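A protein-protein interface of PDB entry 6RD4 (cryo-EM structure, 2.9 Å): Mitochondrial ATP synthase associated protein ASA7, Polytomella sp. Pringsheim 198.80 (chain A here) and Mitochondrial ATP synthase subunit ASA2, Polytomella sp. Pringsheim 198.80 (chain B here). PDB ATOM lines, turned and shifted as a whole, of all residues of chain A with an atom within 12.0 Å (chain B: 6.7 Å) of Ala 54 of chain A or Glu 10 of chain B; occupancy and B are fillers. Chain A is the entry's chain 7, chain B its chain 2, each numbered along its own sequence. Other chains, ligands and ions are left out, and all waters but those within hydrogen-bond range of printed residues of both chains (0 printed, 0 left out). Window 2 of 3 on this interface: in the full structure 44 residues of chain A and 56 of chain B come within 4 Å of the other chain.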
ATOM      1  N   SER A  32     -27.161 -18.879  -6.899  1.00  0.00           N
ATOM      2  CA  SER A  32     -27.877 -17.649  -6.643  1.00  0.00           C
ATOM      3  C   SER A  32     -27.862 -16.786  -7.897  1.00  0.00           C
ATOM      4  O   SER A  32     -27.476 -17.227  -8.983  1.00  0.00           O
ATOM      5  CB  SER A  32     -27.250 -16.900  -5.477  1.00  0.00           C
ATOM      6  OG  SER A  32     -25.989 -16.393  -5.862  1.00  0.00           O
ATOM      7  N   GLY A  33     -28.300 -15.545  -7.750  1.00  0.00           N
ATOM      8  CA  GLY A  33     -28.154 -14.564  -8.800  1.00  0.00           C
ATOM      9  C   GLY A  33     -27.292 -13.418  -8.331  1.00  0.00           C
ATOM     10  O   GLY A  33     -26.937 -12.533  -9.111  1.00  0.00           O
ATOM     11  N   SER A  34     -26.945 -13.434  -7.044  1.00  0.00           N
ATOM     12  CA  SER A  34     -26.148 -12.356  -6.476  1.00  0.00           C
ATOM     13  C   SER A  34     -24.716 -12.406  -6.969  1.00  0.00           C
ATOM     14  O   SER A  34     -24.011 -11.395  -6.939  1.00  0.00           O
ATOM     15  CB  SER A  34     -26.174 -12.437  -4.955  1.00  0.00           C
ATOM     16  OG  SER A  34     -27.486 -12.289  -4.458  1.00  0.00           O
ATOM     17  N   ILE A  35     -24.276 -13.572  -7.415  1.00  0.00           N
ATOM     18  CA  ILE A  35     -22.929 -13.778  -7.921  1.00  0.00           C
ATOM     19  C   ILE A  35     -23.016 -14.823  -9.018  1.00  0.00           C
ATOM     20  O   ILE A  35     -23.685 -15.846  -8.860  1.00  0.00           O
ATOM     21  CB  ILE A  35     -21.976 -14.175  -6.776  1.00  0.00           C
ATOM     22  CG1 ILE A  35     -20.600 -14.559  -7.287  1.00  0.00           C
ATOM     23  CG2 ILE A  35     -22.574 -15.246  -5.887  1.00  0.00           C
ATOM     24  CD1 ILE A  35     -19.603 -14.593  -6.172  1.00  0.00           C
ATOM     25  N   LYS A  36     -22.412 -14.539 -10.162  1.00  0.00           N
ATOM     26  CA  LYS A  36     -22.546 -15.393 -11.329  1.00  0.00           C
ATOM     27  C   LYS A  36     -21.236 -16.127 -11.561  1.00  0.00           C
ATOM     28  O   LYS A  36     -20.206 -15.502 -11.834  1.00  0.00           O
ATOM     29  CB  LYS A  36     -22.957 -14.585 -12.555  1.00  0.00           C
ATOM     30  CG  LYS A  36     -24.457 -14.325 -12.619  1.00  0.00           C
ATOM     31  CD  LYS A  36     -24.814 -13.300 -13.673  1.00  0.00           C
ATOM     32  CE  LYS A  36     -24.373 -11.910 -13.262  1.00  0.00           C
ATOM     33  NZ  LYS A  36     -24.956 -11.505 -11.954  1.00  0.00           N
ATOM     34  N   THR A  49     -15.149 -18.143 -14.539  1.00  0.00           N
ATOM     35  CA  THR A  49     -15.566 -16.769 -14.782  1.00  0.00           C
ATOM     36  C   THR A  49     -16.509 -16.385 -13.656  1.00  0.00           C
ATOM     37  O   THR A  49     -17.614 -16.927 -13.555  1.00  0.00           O
ATOM     38  CB  THR A  49     -16.247 -16.626 -16.139  1.00  0.00           C
ATOM     39  OG1 THR A  49     -15.295 -16.887 -17.177  1.00  0.00           O
ATOM     40  CG2 THR A  49     -16.799 -15.231 -16.309  1.00  0.00           C
ATOM     41  N   VAL A  50     -16.065 -15.481 -12.798  1.00  0.00           N
ATOM     42  CA  VAL A  50     -16.871 -15.033 -11.676  1.00  0.00           C
ATOM     43  C   VAL A  50     -17.323 -13.603 -11.929  1.00  0.00           C
ATOM     44  O   VAL A  50     -16.626 -12.798 -12.559  1.00  0.00           O
ATOM     45  CB  VAL A  50     -16.112 -15.174 -10.340  1.00  0.00           C
ATOM     46  CG1 VAL A  50     -15.700 -16.596 -10.130  1.00  0.00           C
ATOM     47  CG2 VAL A  50     -14.875 -14.373 -10.365  1.00  0.00           C
ATOM     48  N   ALA A  51     -18.526 -13.300 -11.455  1.00  0.00           N
ATOM     49  CA  ALA A  51     -19.154 -12.008 -11.698  1.00  0.00           C
ATOM     50  C   ALA A  51     -19.994 -11.679 -10.479  1.00  0.00           C
ATOM     51  O   ALA A  51     -21.041 -12.294 -10.271  1.00  0.00           O
ATOM     52  CB  ALA A  51     -20.011 -12.050 -12.954  1.00  0.00           C
ATOM     53  N   ALA A  52     -19.539 -10.724  -9.675  1.00  0.00           N
ATOM     54  CA  ALA A  52     -20.234 -10.344  -8.452  1.00  0.00           C
ATOM     55  C   ALA A  52     -20.399  -8.839  -8.440  1.00  0.00           C
ATOM     56  O   ALA A  52     -19.405  -8.110  -8.419  1.00  0.00           O
ATOM     57  CB  ALA A  52     -19.474 -10.801  -7.209  1.00  0.00           C
ATOM     58  N   GLY A  53     -21.644  -8.382  -8.442  1.00  0.00           N
ATOM     59  CA  GLY A  53     -21.889  -6.952  -8.482  1.00  0.00           C
ATOM     60  C   GLY A  53     -21.532  -6.401  -9.842  1.00  0.00           C
ATOM     61  O   GLY A  53     -21.903  -6.958 -10.881  1.00  0.00           O
ATOM     62  N   ALA A  54     -20.785  -5.305  -9.848  1.00  0.00           N
ATOM     63  CA  ALA A  54     -20.287  -4.747 -11.092  1.00  0.00           C
ATOM     64  C   ALA A  54     -18.991  -5.388 -11.547  1.00  0.00           C
ATOM     65  O   ALA A  54     -18.659  -5.309 -12.734  1.00  0.00           O
ATOM     66  CB  ALA A  54     -20.076  -3.239 -10.948  1.00  0.00           C
ATOM     67  N   ALA A  55     -18.263  -6.033 -10.641  1.00  0.00           N
ATOM     68  CA  ALA A  55     -16.936  -6.533 -10.946  1.00  0.00           C
ATOM     69  C   ALA A  55     -17.003  -7.864 -11.677  1.00  0.00           C
ATOM     70  O   ALA A  55     -17.999  -8.588 -11.616  1.00  0.00           O
ATOM     71  CB  ALA A  55     -16.122  -6.691  -9.668  1.00  0.00           C
ATOM     72  N   LYS A  56     -15.925  -8.177 -12.384  1.00  0.00           N
ATOM     73  CA  LYS A  56     -15.778  -9.466 -13.037  1.00  0.00           C
ATOM     74  C   LYS A  56     -14.340  -9.926 -12.905  1.00  0.00           C
ATOM     75  O   LYS A  56     -13.414  -9.117 -12.825  1.00  0.00           O
ATOM     76  CB  LYS A  56     -16.157  -9.417 -14.514  1.00  0.00           C
ATOM     77  CG  LYS A  56     -17.582  -9.817 -14.804  1.00  0.00           C
ATOM     78  CD  LYS A  56     -17.917  -9.613 -16.269  1.00  0.00           C
ATOM     79  CE  LYS A  56     -18.146  -8.147 -16.588  1.00  0.00           C
ATOM     80  NZ  LYS A  56     -19.351  -7.626 -15.890  1.00  0.00           N
ATOM     81  N   ALA A  57     -14.166 -11.236 -12.870  1.00  0.00           N
ATOM     82  CA  ALA A  57     -12.844 -11.824 -12.894  1.00  0.00           C
ATOM     83  C   ALA A  57     -12.938 -13.168 -13.587  1.00  0.00           C
ATOM     84  O   ALA A  57     -13.974 -13.835 -13.528  1.00  0.00           O
ATOM     85  CB  ALA A  57     -12.264 -11.979 -11.489  1.00  0.00           C
ATOM     86  N   ALA A  58     -11.866 -13.538 -14.276  1.00  0.00           N
ATOM     87  CA  ALA A  58     -11.789 -14.827 -14.954  1.00  0.00           C
ATOM     88  C   ALA A  58     -10.321 -15.221 -15.005  1.00  0.00           C
ATOM     89  O   ALA A  58      -9.516 -14.532 -15.634  1.00  0.00           O
ATOM     90  CB  ALA A  58     -12.395 -14.770 -16.349  1.00  0.00           C
ATOM     91  N   GLU B   1     -10.789  -4.670 -16.487  1.00  0.00           N
ATOM     92  CA  GLU B   1     -12.102  -5.285 -16.351  1.00  0.00           C
ATOM     93  C   GLU B   1     -11.982  -6.655 -15.695  1.00  0.00           C
ATOM     94  O   GLU B   1     -12.965  -7.202 -15.200  1.00  0.00           O
ATOM     95  CB  GLU B   1     -12.786  -5.395 -17.713  1.00  0.00           C
ATOM     96  CG  GLU B   1     -12.053  -6.278 -18.694  1.00  0.00           C
ATOM     97  CD  GLU B   1     -12.707  -6.304 -20.050  1.00  0.00           C
ATOM     98  OE1 GLU B   1     -13.751  -5.641 -20.216  1.00  0.00           O
ATOM     99  OE2 GLU B   1     -12.170  -6.981 -20.953  1.00  0.00           O
ATOM    100  N   ASP B   3     -10.974  -7.964 -12.591  1.00  0.00           N
ATOM    101  CA  ASP B   3     -10.806  -7.381 -11.265  1.00  0.00           C
ATOM    102  C   ASP B   3     -10.933  -8.508 -10.256  1.00  0.00           C
ATOM    103  O   ASP B   3     -12.044  -8.965  -9.982  1.00  0.00           O
ATOM    104  CB  ASP B   3     -11.859  -6.306 -11.016  1.00  0.00           C
ATOM    105  CG  ASP B   3     -11.420  -4.935 -11.477  1.00  0.00           C
ATOM    106  OD1 ASP B   3     -12.272  -4.178 -11.984  1.00  0.00           O
ATOM    107  OD2 ASP B   3     -10.230  -4.603 -11.316  1.00  0.00           O
ATOM    108  N   PRO B   5      -9.158  -8.260  -6.858  1.00  0.00           N
ATOM    109  CA  PRO B   5      -9.394  -7.683  -5.526  1.00  0.00           C
ATOM    110  C   PRO B   5     -10.622  -6.806  -5.453  1.00  0.00           C
ATOM    111  O   PRO B   5     -11.123  -6.568  -4.348  1.00  0.00           O
ATOM    112  CB  PRO B   5      -8.125  -6.859  -5.260  1.00  0.00           C
ATOM    113  CG  PRO B   5      -7.190  -7.227  -6.313  1.00  0.00           C
ATOM    114  CD  PRO B   5      -8.060  -7.501  -7.477  1.00  0.00           C
ATOM    115  N   ALA B   6     -11.119  -6.314  -6.575  1.00  0.00           N
ATOM    116  CA  ALA B   6     -12.362  -5.569  -6.576  1.00  0.00           C
ATOM    117  C   ALA B   6     -13.574  -6.469  -6.601  1.00  0.00           C
ATOM    118  O   ALA B   6     -14.684  -5.989  -6.368  1.00  0.00           O
ATOM    119  CB  ALA B   6     -12.420  -4.618  -7.771  1.00  0.00           C
ATOM    120  N   ILE B   7     -13.399  -7.751  -6.911  1.00  0.00           N
ATOM    121  CA  ILE B   7     -14.492  -8.696  -6.751  1.00  0.00           C
ATOM    122  C   ILE B   7     -14.470  -9.336  -5.372  1.00  0.00           C
ATOM    123  O   ILE B   7     -15.473  -9.928  -4.956  1.00  0.00           O
ATOM    124  CB  ILE B   7     -14.486  -9.753  -7.868  1.00  0.00           C
ATOM    125  CG1 ILE B   7     -15.903 -10.209  -8.151  1.00  0.00           C
ATOM    126  CG2 ILE B   7     -13.647 -10.937  -7.527  1.00  0.00           C
ATOM    127  CD1 ILE B   7     -16.016 -11.068  -9.330  1.00  0.00           C
ATOM    128  N   LEU B   8     -13.371  -9.211  -4.637  1.00  0.00           N
ATOM    129  CA  LEU B   8     -13.386  -9.626  -3.246  1.00  0.00           C
ATOM    130  C   LEU B   8     -14.194  -8.662  -2.404  1.00  0.00           C
ATOM    131  O   LEU B   8     -14.878  -9.083  -1.471  1.00  0.00           O
ATOM    132  CB  LEU B   8     -11.970  -9.729  -2.708  1.00  0.00           C
ATOM    133  CG  LEU B   8     -11.149 -10.895  -3.234  1.00  0.00           C
ATOM    134  CD1 LEU B   8      -9.865 -10.951  -2.463  1.00  0.00           C
ATOM    135  CD2 LEU B   8     -11.900 -12.194  -3.126  1.00  0.00           C
ATOM    136  N   LYS B   9     -14.143  -7.372  -2.731  1.00  0.00           N
ATOM    137  CA  LYS B   9     -14.947  -6.383  -2.025  1.00  0.00           C
ATOM    138  C   LYS B   9     -16.416  -6.496  -2.405  1.00  0.00           C
ATOM    139  O   LYS B   9     -17.291  -6.111  -1.630  1.00  0.00           O
ATOM    140  CB  LYS B   9     -14.407  -4.988  -2.319  1.00  0.00           C
ATOM    141  CG  LYS B   9     -14.958  -3.904  -1.425  1.00  0.00           C
ATOM    142  CD  LYS B   9     -14.296  -2.562  -1.665  1.00  0.00           C
ATOM    143  CE  LYS B   9     -14.822  -1.902  -2.910  1.00  0.00           C
ATOM    144  NZ  LYS B   9     -14.265  -0.535  -3.029  1.00  0.00           N
ATOM    145  N   GLU B  10     -16.712  -7.031  -3.581  1.00  0.00           N
ATOM    146  CA  GLU B  10     -18.101  -7.264  -3.934  1.00  0.00           C
ATOM    147  C   GLU B  10     -18.632  -8.562  -3.356  1.00  0.00           C
ATOM    148  O   GLU B  10     -19.851  -8.730  -3.268  1.00  0.00           O
ATOM    149  CB  GLU B  10     -18.266  -7.257  -5.447  1.00  0.00           C
ATOM    150  CG  GLU B  10     -18.180  -5.882  -6.068  1.00  0.00           C
ATOM    151  CD  GLU B  10     -19.292  -4.970  -5.593  1.00  0.00           C
ATOM    152  OE1 GLU B  10     -19.032  -4.095  -4.739  1.00  0.00           O
ATOM    153  OE2 GLU B  10     -20.434  -5.135  -6.066  1.00  0.00           O
ATOM    154  N   ILE B  11     -17.748  -9.495  -3.003  1.00  0.00           N
ATOM    155  CA  ILE B  11     -18.155 -10.681  -2.257  1.00  0.00           C
ATOM    156  C   ILE B  11     -18.275 -10.342  -0.779  1.00  0.00           C
ATOM    157  O   ILE B  11     -19.190 -10.819  -0.101  1.00  0.00           O
ATOM    158  CB  ILE B  11     -17.162 -11.830  -2.516  1.00  0.00           C
ATOM    159  CG1 ILE B  11     -17.350 -12.390  -3.915  1.00  0.00           C
ATOM    160  CG2 ILE B  11     -17.337 -12.969  -1.550  1.00  0.00           C
ATOM    161  CD1 ILE B  11     -16.242 -13.304  -4.339  1.00  0.00           C
ATOM    162  N   ASP B  12     -17.388  -9.476  -0.285  1.00  0.00           N
ATOM    163  CA  ASP B  12     -17.421  -9.046   1.106  1.00  0.00           C
ATOM    164  C   ASP B  12     -18.711  -8.308   1.418  1.00  0.00           C
ATOM    165  O   ASP B  12     -19.286  -8.492   2.490  1.00  0.00           O
ATOM    166  CB  ASP B  12     -16.188  -8.181   1.384  1.00  0.00           C
ATOM    167  CG  ASP B  12     -16.010  -7.804   2.849  1.00  0.00           C
ATOM    168  OD1 ASP B  12     -14.932  -8.118   3.394  1.00  0.00           O
ATOM    169  OD2 ASP B  12     -16.862  -7.112   3.441  1.00  0.00           O
ATOM    170  N   SER B  13     -19.208  -7.504   0.490  1.00  0.00           N
ATOM    171  CA  SER B  13     -20.485  -6.846   0.710  1.00  0.00           C
ATOM    172  C   SER B  13     -21.671  -7.746   0.426  1.00  0.00           C
ATOM    173  O   SER B  13     -22.804  -7.339   0.680  1.00  0.00           O
ATOM    174  CB  SER B  13     -20.583  -5.591  -0.144  1.00  0.00           C
ATOM    175  OG  SER B  13     -19.443  -4.772   0.047  1.00  0.00           O
ATOM    176  N   LEU B  14     -21.458  -8.940  -0.105  1.00  0.00           N
ATOM    177  CA  LEU B  14     -22.566  -9.872  -0.247  1.00  0.00           C
ATOM    178  C   LEU B  14     -22.807 -10.633   1.048  1.00  0.00           C
ATOM    179  O   LEU B  14     -23.952 -10.919   1.399  1.00  0.00           O
ATOM    180  CB  LEU B  14     -22.296 -10.831  -1.403  1.00  0.00           C
ATOM    181  CG  LEU B  14     -23.045 -12.159  -1.471  1.00  0.00           C
ATOM    182  CD1 LEU B  14     -24.514 -11.952  -1.694  1.00  0.00           C
ATOM    183  CD2 LEU B  14     -22.480 -13.022  -2.561  1.00  0.00           C
ATOM    184  N   VAL B  15     -21.740 -10.962   1.777  1.00  0.00           N
ATOM    185  CA  VAL B  15     -21.866 -11.716   3.012  1.00  0.00           C
ATOM    186  C   VAL B  15     -21.857 -10.832   4.237  1.00  0.00           C
ATOM    187  O   VAL B  15     -21.993 -11.344   5.348  1.00  0.00           O
ATOM    188  CB  VAL B  15     -20.763 -12.783   3.134  1.00  0.00           C
ATOM    189  CG1 VAL B  15     -20.920 -13.817   2.063  1.00  0.00           C
ATOM    190  CG2 VAL B  15     -19.420 -12.144   3.050  1.00  0.00           C
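CD1 of Leu 14 of chain B touches CB of Ser 34 of chain A, at 3.7 Å.
CD1 of Ile 35 of chain A touches CG1 of Ile 11 of chain B, at 3.9 Å.
CD1 of Ile 7 of chain B touches CG2 of Val 50 of chain A, at 3.6 Å.
Ala 51 of chain A touches Ile 7 of chain B (N to CD1, 3.97 Å).
Glu 10 of chain B touches Ala 52 of chain A (CB to O, 3.3 Å).
OE2 of Glu 10 of chain B touches CA of Gly 53 of chain A, 3.4 Å away.
Glu 10 of chain B touches Ala 54 of chain A (OE2 to N, 3.8 Å).
Ala 6 of chain B touches Ala 55 of chain A.
CG1 of Ile 7 of chain B touches CB of Ala 55 of chain A, 3.8 Å away.
O of Asp 3 of chain B touches CB of Ala 57 of chain A, 3.4 Å away.
Of chain B, only Glu 10 (3.8 Å) comes within 4 Å of Ala 54 of chain A.
Of the printed residues of chain A, Glu 10 of chain B touches Ala 52, Gly 53 and Ala 54.
Asp 12 of chain B touches none of the printed residues of chain A.
No residue of chain A comes within 4 Å of Ser 13 of chain B.
Of the printed residues of chain B, Ile 35 of chain A touches Ile 11 (3.9 Å).
Of the printed residues of chain B, Val 50 of chain A touches Ile 7 (3.6 Å).
Of the printed residues of chain B, Ala 57 of chain A touches Asp 3 and Ile 7.
Printed residues of chain B within 4 Å of Gly 53 of chain A: Glu 10.
Thr 49 of chain A touches none of the printed residues of chain B.
The nearest residue of chain B that does not touch Ala 54 of chain A is Glu 1 of chain B (6.5 Å).
The nearest residue of chain A that does not touch Glu 10 of chain B is Ala 55 of chain A (4.2 Å).
The nearest printed residue of chain A that does not touch Leu 14 of chain B is Ile 35 of chain A (4.002 Å).
The backbone carbonyl oxygen of Glu 1 of chain B sits close to the backbone carbonyl oxygen of Lys 56 of chain A, at 3.1 Å.
N of Asp 3 of chain B lies within hydrogen-bond range of O of Lys 56 of chain A (2.7 Å).
N of Val 50 of chain A sits at hydrogen-bond distance from O of Ala 57 of chain A (2.8 Å).
The backbone NH (N) of Lys 36 of chain A sits at hydrogen-bond distance from the backbone carbonyl oxygen (O) of Ala 51 of chain A (2.6 Å).
The side-chain hydroxyl (OG) of Ser 32 of chain A lies within hydrogen-bond range of the backbone NH (N) of Ser 34 of chain A, 3.3 Å away.
Printed residues of chain A that touch a printed residue of chain B: Ser 34, Ile 35, Val 50, Ala 51, Ala 52, Gly 53, Ala 54, Ala 55, Lys 56 and Ala 57.
Hydrophobic or aromatic side chains of chain A within 4 Å of the printed part of chain B: Ile 35, Val 50, Ala 52, Ala 55 and Ala 57.
Hydrophobic or aromatic side chains of chain B that line the printed part of chain A: Ile 7, Ile 11 and Leu 14.
Among the printed residues, no Asp or Glu carboxylate lies within 4 Å of a Lys or Arg side-chain nitrogen of the other chain.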
